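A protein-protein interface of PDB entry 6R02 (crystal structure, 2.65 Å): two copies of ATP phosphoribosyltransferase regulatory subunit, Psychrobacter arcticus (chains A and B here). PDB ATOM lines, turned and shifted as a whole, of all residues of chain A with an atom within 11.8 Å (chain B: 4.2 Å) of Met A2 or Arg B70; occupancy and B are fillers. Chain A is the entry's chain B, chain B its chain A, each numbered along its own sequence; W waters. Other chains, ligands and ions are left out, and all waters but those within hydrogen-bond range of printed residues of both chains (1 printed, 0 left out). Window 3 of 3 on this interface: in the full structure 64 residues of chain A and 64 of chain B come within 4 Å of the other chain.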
ATOM      1  N   GLY A   1     -21.124   4.753  13.744  1.00  0.00           N
ATOM      2  CA  GLY A   1     -20.029   4.078  12.984  1.00  0.00           C
ATOM      3  C   GLY A   1     -18.729   4.017  13.774  1.00  0.00           C
ATOM      4  O   GLY A   1     -18.788   3.932  15.014  1.00  0.00           O
ATOM      5  N   MET A   2     -17.599   4.035  13.063  1.00  0.00           N
ATOM      6  CA  MET A   2     -16.217   3.952  13.608  1.00  0.00           C
ATOM      7  C   MET A   2     -15.891   5.248  14.370  1.00  0.00           C
ATOM      8  O   MET A   2     -16.436   6.307  13.986  1.00  0.00           O
ATOM      9  CB  MET A   2     -15.246   3.736  12.440  1.00  0.00           C
ATOM     10  CG  MET A   2     -13.792   3.982  12.748  1.00  0.00           C
ATOM     11  SD  MET A   2     -12.711   3.397  11.415  1.00  0.00           S
ATOM     12  CE  MET A   2     -13.409   4.251  10.002  1.00  0.00           C
ATOM     13  N   LEU A   3     -15.050   5.163  15.406  1.00  0.00           N
ATOM     14  CA  LEU A   3     -14.600   6.327  16.219  1.00  0.00           C
ATOM     15  C   LEU A   3     -13.134   6.630  15.924  1.00  0.00           C
ATOM     16  O   LEU A   3     -12.401   5.758  15.469  1.00  0.00           O
ATOM     17  CB  LEU A   3     -14.797   6.024  17.709  1.00  0.00           C
ATOM     18  CG  LEU A   3     -16.235   6.041  18.215  1.00  0.00           C
ATOM     19  CD1 LEU A   3     -16.300   5.465  19.620  1.00  0.00           C
ATOM     20  CD2 LEU A   3     -16.813   7.452  18.212  1.00  0.00           C
ATOM     21  N   PRO A   4     -12.658   7.874  16.166  1.00  0.00           N
ATOM     22  CA  PRO A   4     -11.261   8.218  15.912  1.00  0.00           C
ATOM     23  C   PRO A   4     -10.326   7.456  16.863  1.00  0.00           C
ATOM     24  O   PRO A   4     -10.723   7.186  17.971  1.00  0.00           O
ATOM     25  CB  PRO A   4     -11.181   9.731  16.160  1.00  0.00           C
ATOM     26  CG  PRO A   4     -12.624  10.201  16.196  1.00  0.00           C
ATOM     27  CD  PRO A   4     -13.423   9.015  16.693  1.00  0.00           C
ATOM     28  N   ASP A   5      -9.117   7.129  16.401  1.00  0.00           N
ATOM     29  CA  ASP A   5      -8.080   6.436  17.206  1.00  0.00           C
ATOM     30  C   ASP A   5      -7.869   7.230  18.500  1.00  0.00           C
ATOM     31  O   ASP A   5      -7.727   8.464  18.418  1.00  0.00           O
ATOM     32  CB  ASP A   5      -6.779   6.264  16.420  1.00  0.00           C
ATOM     33  CG  ASP A   5      -6.846   5.206  15.332  1.00  0.00           C
ATOM     34  OD1 ASP A   5      -7.956   4.721  15.038  1.00  0.00           O
ATOM     35  OD2 ASP A   5      -5.775   4.861  14.789  1.00  0.00           O
ATOM     36  N   GLY A   6      -7.879   6.537  19.646  1.00  0.00           N
ATOM     37  CA  GLY A   6      -7.680   7.129  20.982  1.00  0.00           C
ATOM     38  C   GLY A   6      -8.939   7.783  21.522  1.00  0.00           C
ATOM     39  O   GLY A   6      -8.828   8.578  22.459  1.00  0.00           O
ATOM     40  N   VAL A   7     -10.095   7.480  20.933  1.00  0.00           N
ATOM     41  CA  VAL A   7     -11.427   7.975  21.390  1.00  0.00           C
ATOM     42  C   VAL A   7     -12.332   6.756  21.565  1.00  0.00           C
ATOM     43  O   VAL A   7     -12.512   6.014  20.573  1.00  0.00           O
ATOM     44  CB  VAL A   7     -12.030   8.986  20.397  1.00  0.00           C
ATOM     45  CG1 VAL A   7     -13.403   9.445  20.840  1.00  0.00           C
ATOM     46  CG2 VAL A   7     -11.121  10.184  20.178  1.00  0.00           C
ATOM     47  N   ALA A   8     -12.874   6.552  22.769  1.00  0.00           N
ATOM     48  CA  ALA A   8     -13.682   5.362  23.118  1.00  0.00           C
ATOM     49  C   ALA A   8     -14.923   5.769  23.914  1.00  0.00           C
ATOM     50  O   ALA A   8     -14.830   6.695  24.731  1.00  0.00           O
ATOM     51  CB  ALA A   8     -12.836   4.381  23.885  1.00  0.00           C
ATOM     52  N   ASP A   9     -16.044   5.101  23.659  1.00  0.00           N
ATOM     53  CA  ASP A   9     -17.218   5.113  24.569  1.00  0.00           C
ATOM     54  C   ASP A   9     -16.790   4.435  25.872  1.00  0.00           C
ATOM     55  O   ASP A   9     -16.069   3.417  25.794  1.00  0.00           O
ATOM     56  CB  ASP A   9     -18.420   4.343  24.018  1.00  0.00           C
ATOM     57  CG  ASP A   9     -18.975   4.848  22.706  1.00  0.00           C
ATOM     58  OD1 ASP A   9     -19.153   6.079  22.593  1.00  0.00           O
ATOM     59  OD2 ASP A   9     -19.220   4.002  21.812  1.00  0.00           O
ATOM     60  N   PHE A  61      -6.153  21.394  20.434  1.00  0.00           N
ATOM     61  CA  PHE A  61      -7.046  21.722  19.292  1.00  0.00           C
ATOM     62  C   PHE A  61      -7.389  23.215  19.351  1.00  0.00           C
ATOM     63  O   PHE A  61      -7.658  23.714  20.455  1.00  0.00           O
ATOM     64  CB  PHE A  61      -8.334  20.896  19.335  1.00  0.00           C
ATOM     65  CG  PHE A  61      -8.199  19.482  18.833  1.00  0.00           C
ATOM     66  CD1 PHE A  61      -8.063  19.230  17.478  1.00  0.00           C
ATOM     67  CD2 PHE A  61      -8.228  18.407  19.708  1.00  0.00           C
ATOM     68  CE1 PHE A  61      -7.943  17.932  17.008  1.00  0.00           C
ATOM     69  CE2 PHE A  61      -8.102  17.110  19.239  1.00  0.00           C
ATOM     70  CZ  PHE A  61      -7.961  16.874  17.889  1.00  0.00           C
ATOM     71  N   LYS A  62      -7.375  23.891  18.200  1.00  0.00           N
ATOM     72  CA  LYS A  62      -7.730  25.328  18.052  1.00  0.00           C
ATOM     73  C   LYS A  62      -9.099  25.454  17.377  1.00  0.00           C
ATOM     74  O   LYS A  62      -9.393  24.645  16.479  1.00  0.00           O
ATOM     75  CB  LYS A  62      -6.663  26.052  17.227  1.00  0.00           C
ATOM     76  CG  LYS A  62      -5.528  26.669  18.028  1.00  0.00           C
ATOM     77  CD  LYS A  62      -4.557  25.661  18.580  1.00  0.00           C
ATOM     78  CE  LYS A  62      -3.381  26.318  19.272  1.00  0.00           C
ATOM     79  NZ  LYS A  62      -2.297  25.342  19.537  1.00  0.00           N
ATOM     80  N   HIS A 105      -6.558  15.782  23.638  1.00  0.00           N
ATOM     81  CA  HIS A 105      -5.220  15.873  22.996  1.00  0.00           C
ATOM     82  C   HIS A 105      -5.382  15.676  21.487  1.00  0.00           C
ATOM     83  O   HIS A 105      -6.224  14.859  21.092  1.00  0.00           O
ATOM     84  CB  HIS A 105      -4.247  14.858  23.601  1.00  0.00           C
ATOM     85  CG  HIS A 105      -4.061  15.011  25.070  1.00  0.00           C
ATOM     86  ND1 HIS A 105      -3.605  13.980  25.864  1.00  0.00           N
ATOM     87  CD2 HIS A 105      -4.272  16.067  25.887  1.00  0.00           C
ATOM     88  CE1 HIS A 105      -3.547  14.396  27.118  1.00  0.00           C
ATOM     89  NE2 HIS A 105      -3.930  15.684  27.155  1.00  0.00           N
ATOM     90  N   THR A 106      -4.618  16.414  20.684  1.00  0.00           N
ATOM     91  CA  THR A 106      -4.610  16.305  19.206  1.00  0.00           C
ATOM     92  C   THR A 106      -4.048  14.936  18.823  1.00  0.00           C
ATOM     93  O   THR A 106      -4.598  14.317  17.900  1.00  0.00           O
ATOM     94  CB  THR A 106      -3.808  17.441  18.562  1.00  0.00           C
ATOM     95  OG1 THR A 106      -2.461  17.317  19.018  1.00  0.00           O
ATOM     96  CG2 THR A 106      -4.362  18.815  18.879  1.00  0.00           C
ATOM     97  N   LEU A 107      -2.999  14.490  19.514  1.00  0.00           N
ATOM     98  CA  LEU A 107      -2.320  13.190  19.263  1.00  0.00           C
ATOM     99  C   LEU A 107      -2.307  12.350  20.537  1.00  0.00           C
ATOM    100  O   LEU A 107      -2.317  12.896  21.639  1.00  0.00           O
ATOM    101  CB  LEU A 107      -0.895  13.458  18.775  1.00  0.00           C
ATOM    102  CG  LEU A 107      -0.793  14.069  17.377  1.00  0.00           C
ATOM    103  CD1 LEU A 107       0.611  14.582  17.109  1.00  0.00           C
ATOM    104  CD2 LEU A 107      -1.209  13.066  16.312  1.00  0.00           C
ATOM    105  N   ARG A 115      -6.949   9.976  23.757  1.00  0.00           N
ATOM    106  CA  ARG A 115      -6.872  11.418  23.422  1.00  0.00           C
ATOM    107  C   ARG A 115      -7.931  12.173  24.234  1.00  0.00           C
ATOM    108  O   ARG A 115      -8.010  13.410  24.091  1.00  0.00           O
ATOM    109  CB  ARG A 115      -7.083  11.625  21.921  1.00  0.00           C
ATOM    110  CG  ARG A 115      -5.843  11.384  21.071  1.00  0.00           C
ATOM    111  CD  ARG A 115      -5.959  11.974  19.671  1.00  0.00           C
ATOM    112  NE  ARG A 115      -6.832  11.209  18.790  1.00  0.00           N
ATOM    113  CZ  ARG A 115      -7.045  11.484  17.513  1.00  0.00           C
ATOM    114  NH1 ARG A 115      -6.441  12.502  16.931  1.00  0.00           N
ATOM    115  NH2 ARG A 115      -7.858  10.722  16.807  1.00  0.00           N
ATOM    116  N   PHE B  44     -15.885  11.711  14.733  1.00  0.00           N
ATOM    117  CA  PHE B  44     -15.970  12.120  13.307  1.00  0.00           C
ATOM    118  C   PHE B  44     -17.363  12.706  13.059  1.00  0.00           C
ATOM    119  O   PHE B  44     -18.326  12.222  13.685  1.00  0.00           O
ATOM    120  CB  PHE B  44     -15.691  10.927  12.395  1.00  0.00           C
ATOM    121  CG  PHE B  44     -14.284  10.386  12.470  1.00  0.00           C
ATOM    122  CD1 PHE B  44     -13.194  11.225  12.324  1.00  0.00           C
ATOM    123  CD2 PHE B  44     -14.050   9.032  12.648  1.00  0.00           C
ATOM    124  CE1 PHE B  44     -11.900  10.726  12.365  1.00  0.00           C
ATOM    125  CE2 PHE B  44     -12.757   8.535  12.691  1.00  0.00           C
ATOM    126  CZ  PHE B  44     -11.684   9.382  12.548  1.00  0.00           C
ATOM    127  N   GLU B  46     -19.245  12.457  10.485  1.00  0.00           N
ATOM    128  CA  GLU B  46     -20.032  11.356   9.860  1.00  0.00           C
ATOM    129  C   GLU B  46     -20.975  10.717  10.886  1.00  0.00           C
ATOM    130  O   GLU B  46     -22.125  10.442  10.518  1.00  0.00           O
ATOM    131  CB  GLU B  46     -19.115  10.271   9.285  1.00  0.00           C
ATOM    132  CG  GLU B  46     -18.561  10.594   7.908  1.00  0.00           C
ATOM    133  CD  GLU B  46     -17.338  11.496   7.867  1.00  0.00           C
ATOM    134  OE1 GLU B  46     -16.790  11.823   8.954  1.00  0.00           O
ATOM    135  OE2 GLU B  46     -16.930  11.867   6.740  1.00  0.00           O
ATOM    136  N   ILE B  64      -9.677  19.068  13.294  1.00  0.00           N
ATOM    137  CA  ILE B  64      -9.040  18.180  12.277  1.00  0.00           C
ATOM    138  C   ILE B  64      -8.348  17.029  13.005  1.00  0.00           C
ATOM    139  O   ILE B  64      -7.455  17.313  13.834  1.00  0.00           O
ATOM    140  CB  ILE B  64      -8.016  18.962  11.432  1.00  0.00           C
ATOM    141  CG1 ILE B  64      -8.457  20.400  11.135  1.00  0.00           C
ATOM    142  CG2 ILE B  64      -7.688  18.179  10.173  1.00  0.00           C
ATOM    143  CD1 ILE B  64      -9.725  20.506  10.318  1.00  0.00           C
ATOM    144  N   ASP B  65      -8.711  15.784  12.700  1.00  0.00           N
ATOM    145  CA  ASP B  65      -7.966  14.595  13.189  1.00  0.00           C
ATOM    146  C   ASP B  65      -6.667  14.502  12.389  1.00  0.00           C
ATOM    147  O   ASP B  65      -6.742  14.179  11.206  1.00  0.00           O
ATOM    148  CB  ASP B  65      -8.768  13.302  13.054  1.00  0.00           C
ATOM    149  CG  ASP B  65      -7.950  12.060  13.368  1.00  0.00           C
ATOM    150  OD1 ASP B  65      -6.863  12.213  13.972  1.00  0.00           O
ATOM    151  OD2 ASP B  65      -8.405  10.950  13.001  1.00  0.00           O
ATOM    152  N   THR B  68      -5.779  11.027  10.416  1.00  0.00           N
ATOM    153  CA  THR B  68      -6.530  10.621   9.196  1.00  0.00           C
ATOM    154  C   THR B  68      -6.738  11.795   8.228  1.00  0.00           C
ATOM    155  O   THR B  68      -6.988  11.520   7.043  1.00  0.00           O
ATOM    156  CB  THR B  68      -7.887  10.023   9.577  1.00  0.00           C
ATOM    157  OG1 THR B  68      -8.619  11.017  10.297  1.00  0.00           O
ATOM    158  CG2 THR B  68      -7.758   8.764  10.406  1.00  0.00           C
ATOM    159  N   GLY B  69      -6.679  13.039   8.711  1.00  0.00           N
ATOM    160  CA  GLY B  69      -6.995  14.250   7.927  1.00  0.00           C
ATOM    161  C   GLY B  69      -8.487  14.554   7.919  1.00  0.00           C
ATOM    162  O   GLY B  69      -8.864  15.606   7.379  1.00  0.00           O
ATOM    163  N   ARG B  70      -9.307  13.688   8.525  1.00  0.00           N
ATOM    164  CA  ARG B  70     -10.788  13.777   8.498  1.00  0.00           C
ATOM    165  C   ARG B  70     -11.285  14.813   9.510  1.00  0.00           C
ATOM    166  O   ARG B  70     -10.563  15.104  10.479  1.00  0.00           O
ATOM    167  CB  ARG B  70     -11.404  12.414   8.814  1.00  0.00           C
ATOM    168  CG  ARG B  70     -11.038  11.325   7.814  1.00  0.00           C
ATOM    169  CD  ARG B  70     -11.646   9.981   8.161  1.00  0.00           C
ATOM    170  NE  ARG B  70     -13.058  10.095   8.492  1.00  0.00           N
ATOM    171  CZ  ARG B  70     -13.808   9.110   8.969  1.00  0.00           C
ATOM    172  NH1 ARG B  70     -13.284   7.914   9.181  1.00  0.00           N
ATOM    173  NH2 ARG B  70     -15.085   9.328   9.231  1.00  0.00           N
ATOM    174  N   LEU B  71     -12.502  15.316   9.297  1.00  0.00           N
ATOM    175  CA  LEU B  71     -13.174  16.292  10.193  1.00  0.00           C
ATOM    176  C   LEU B  71     -13.738  15.555  11.406  1.00  0.00           C
ATOM    177  O   LEU B  71     -14.323  14.470  11.229  1.00  0.00           O
ATOM    178  CB  LEU B  71     -14.297  17.007   9.437  1.00  0.00           C
ATOM    179  CG  LEU B  71     -13.849  18.071   8.438  1.00  0.00           C
ATOM    180  CD1 LEU B  71     -14.983  18.436   7.491  1.00  0.00           C
ATOM    181  CD2 LEU B  71     -13.331  19.309   9.154  1.00  0.00           C
ATOM    182  N   MET B  72     -13.564  16.141  12.590  1.00  0.00           N
ATOM    183  CA  MET B  72     -14.236  15.733  13.849  1.00  0.00           C
ATOM    184  C   MET B  72     -15.036  16.931  14.363  1.00  0.00           C
ATOM    185  O   MET B  72     -14.880  18.023  13.801  1.00  0.00           O
ATOM    186  CB  MET B  72     -13.212  15.298  14.899  1.00  0.00           C
ATOM    187  CG  MET B  72     -12.314  14.169  14.429  1.00  0.00           C
ATOM    188  SD  MET B  72     -11.252  13.507  15.732  1.00  0.00           S
ATOM    189  CE  MET B  72     -10.294  14.961  16.151  1.00  0.00           C
HETATM  190  O   HOH W   1     -17.345   7.445  10.892  1.00  0.00           O
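Of the 15 printed residues of chain A, 5 touch a printed residue of chain B. Hydrophobic or aromatic side chains of chain A within 4 Å of the printed part of chain B: Met A2, Pro A4 and Phe A61. Of the 9 printed residues of chain B, 5 touch a printed residue of chain A. Among the printed residues, 8 pairs touch across the chains. Among the printed residues, Asp or Glu carboxylates within 4 Å of a Lys or Arg side-chain nitrogen of the other chain: Arg A115 with Asp B65.
The side-chain carboxylate (OD1) of Asp B65 is in salt-bridge range of the guanidinium group (NH1) of Arg A115 (3.0 Å).
Met A2 touches just these residues of chain B: Phe B44 and Arg B70. Printed residues of chain B within 4 Å of Phe A61: Ile B64 (3.3 Å) and Met B72 (3.5 Å). Of the printed residues of chain B, Arg A115 touches Asp B65 (3.0 Å). Phe B44 touches three residues of chain A. Glu B46 touches none of the printed residues of chain A. Of chain A, only Arg A115 comes within 4 Å of Asp B65. Arg B70 touches just one residue of chain A: Met A2. No residue of chain A comes within 4 Å of Leu B71. Met B72 touches two residues of chain A. The nearest printed residue of chain B that does not touch Met A2 is Glu B46 (6.7 Å). The nearest residue of chain A that does not touch Arg B70 is Leu A3 (6.7 Å).
NH2 of Arg B70 lies within salt-bridge range of OE1 of Glu B46 (3.0 Å). The side-chain hydroxyl (OG1) of Thr B68 is in hydrogen-bond range of the side-chain carboxylate (OD2) of Asp B65. The backbone NH (N) of Asp B65 is in hydrogen-bond range of the backbone carbonyl oxygen (O) of Arg B70. O of Asp A5 is in hydrogen-bond range of NH2 of Arg A115 (2.8 Å). N of Arg A115 is in hydrogen-bond range of O of Gly A6 (2.7 Å). N of His A105 is in hydrogen-bond range of O of Arg A115.
Met A2 touches Phe B44 (O to CD2, 3.9 Å). Met A2 touches Arg B70 (CE to NH1, 3.8 Å). C of Leu A3 touches CE2 of Phe B44 (3.8 Å). Pro A4 touches Phe B44 (N to CE2, 3.5 Å). Pro A4 touches Met B72. Ile B64 touches Phe A61 (O to CE1, 3.3 Å). Phe A61 touches Met B72.
Water W1 bridges NH2 of Arg B70 and O of Met A2.
No position is printed for both chains.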
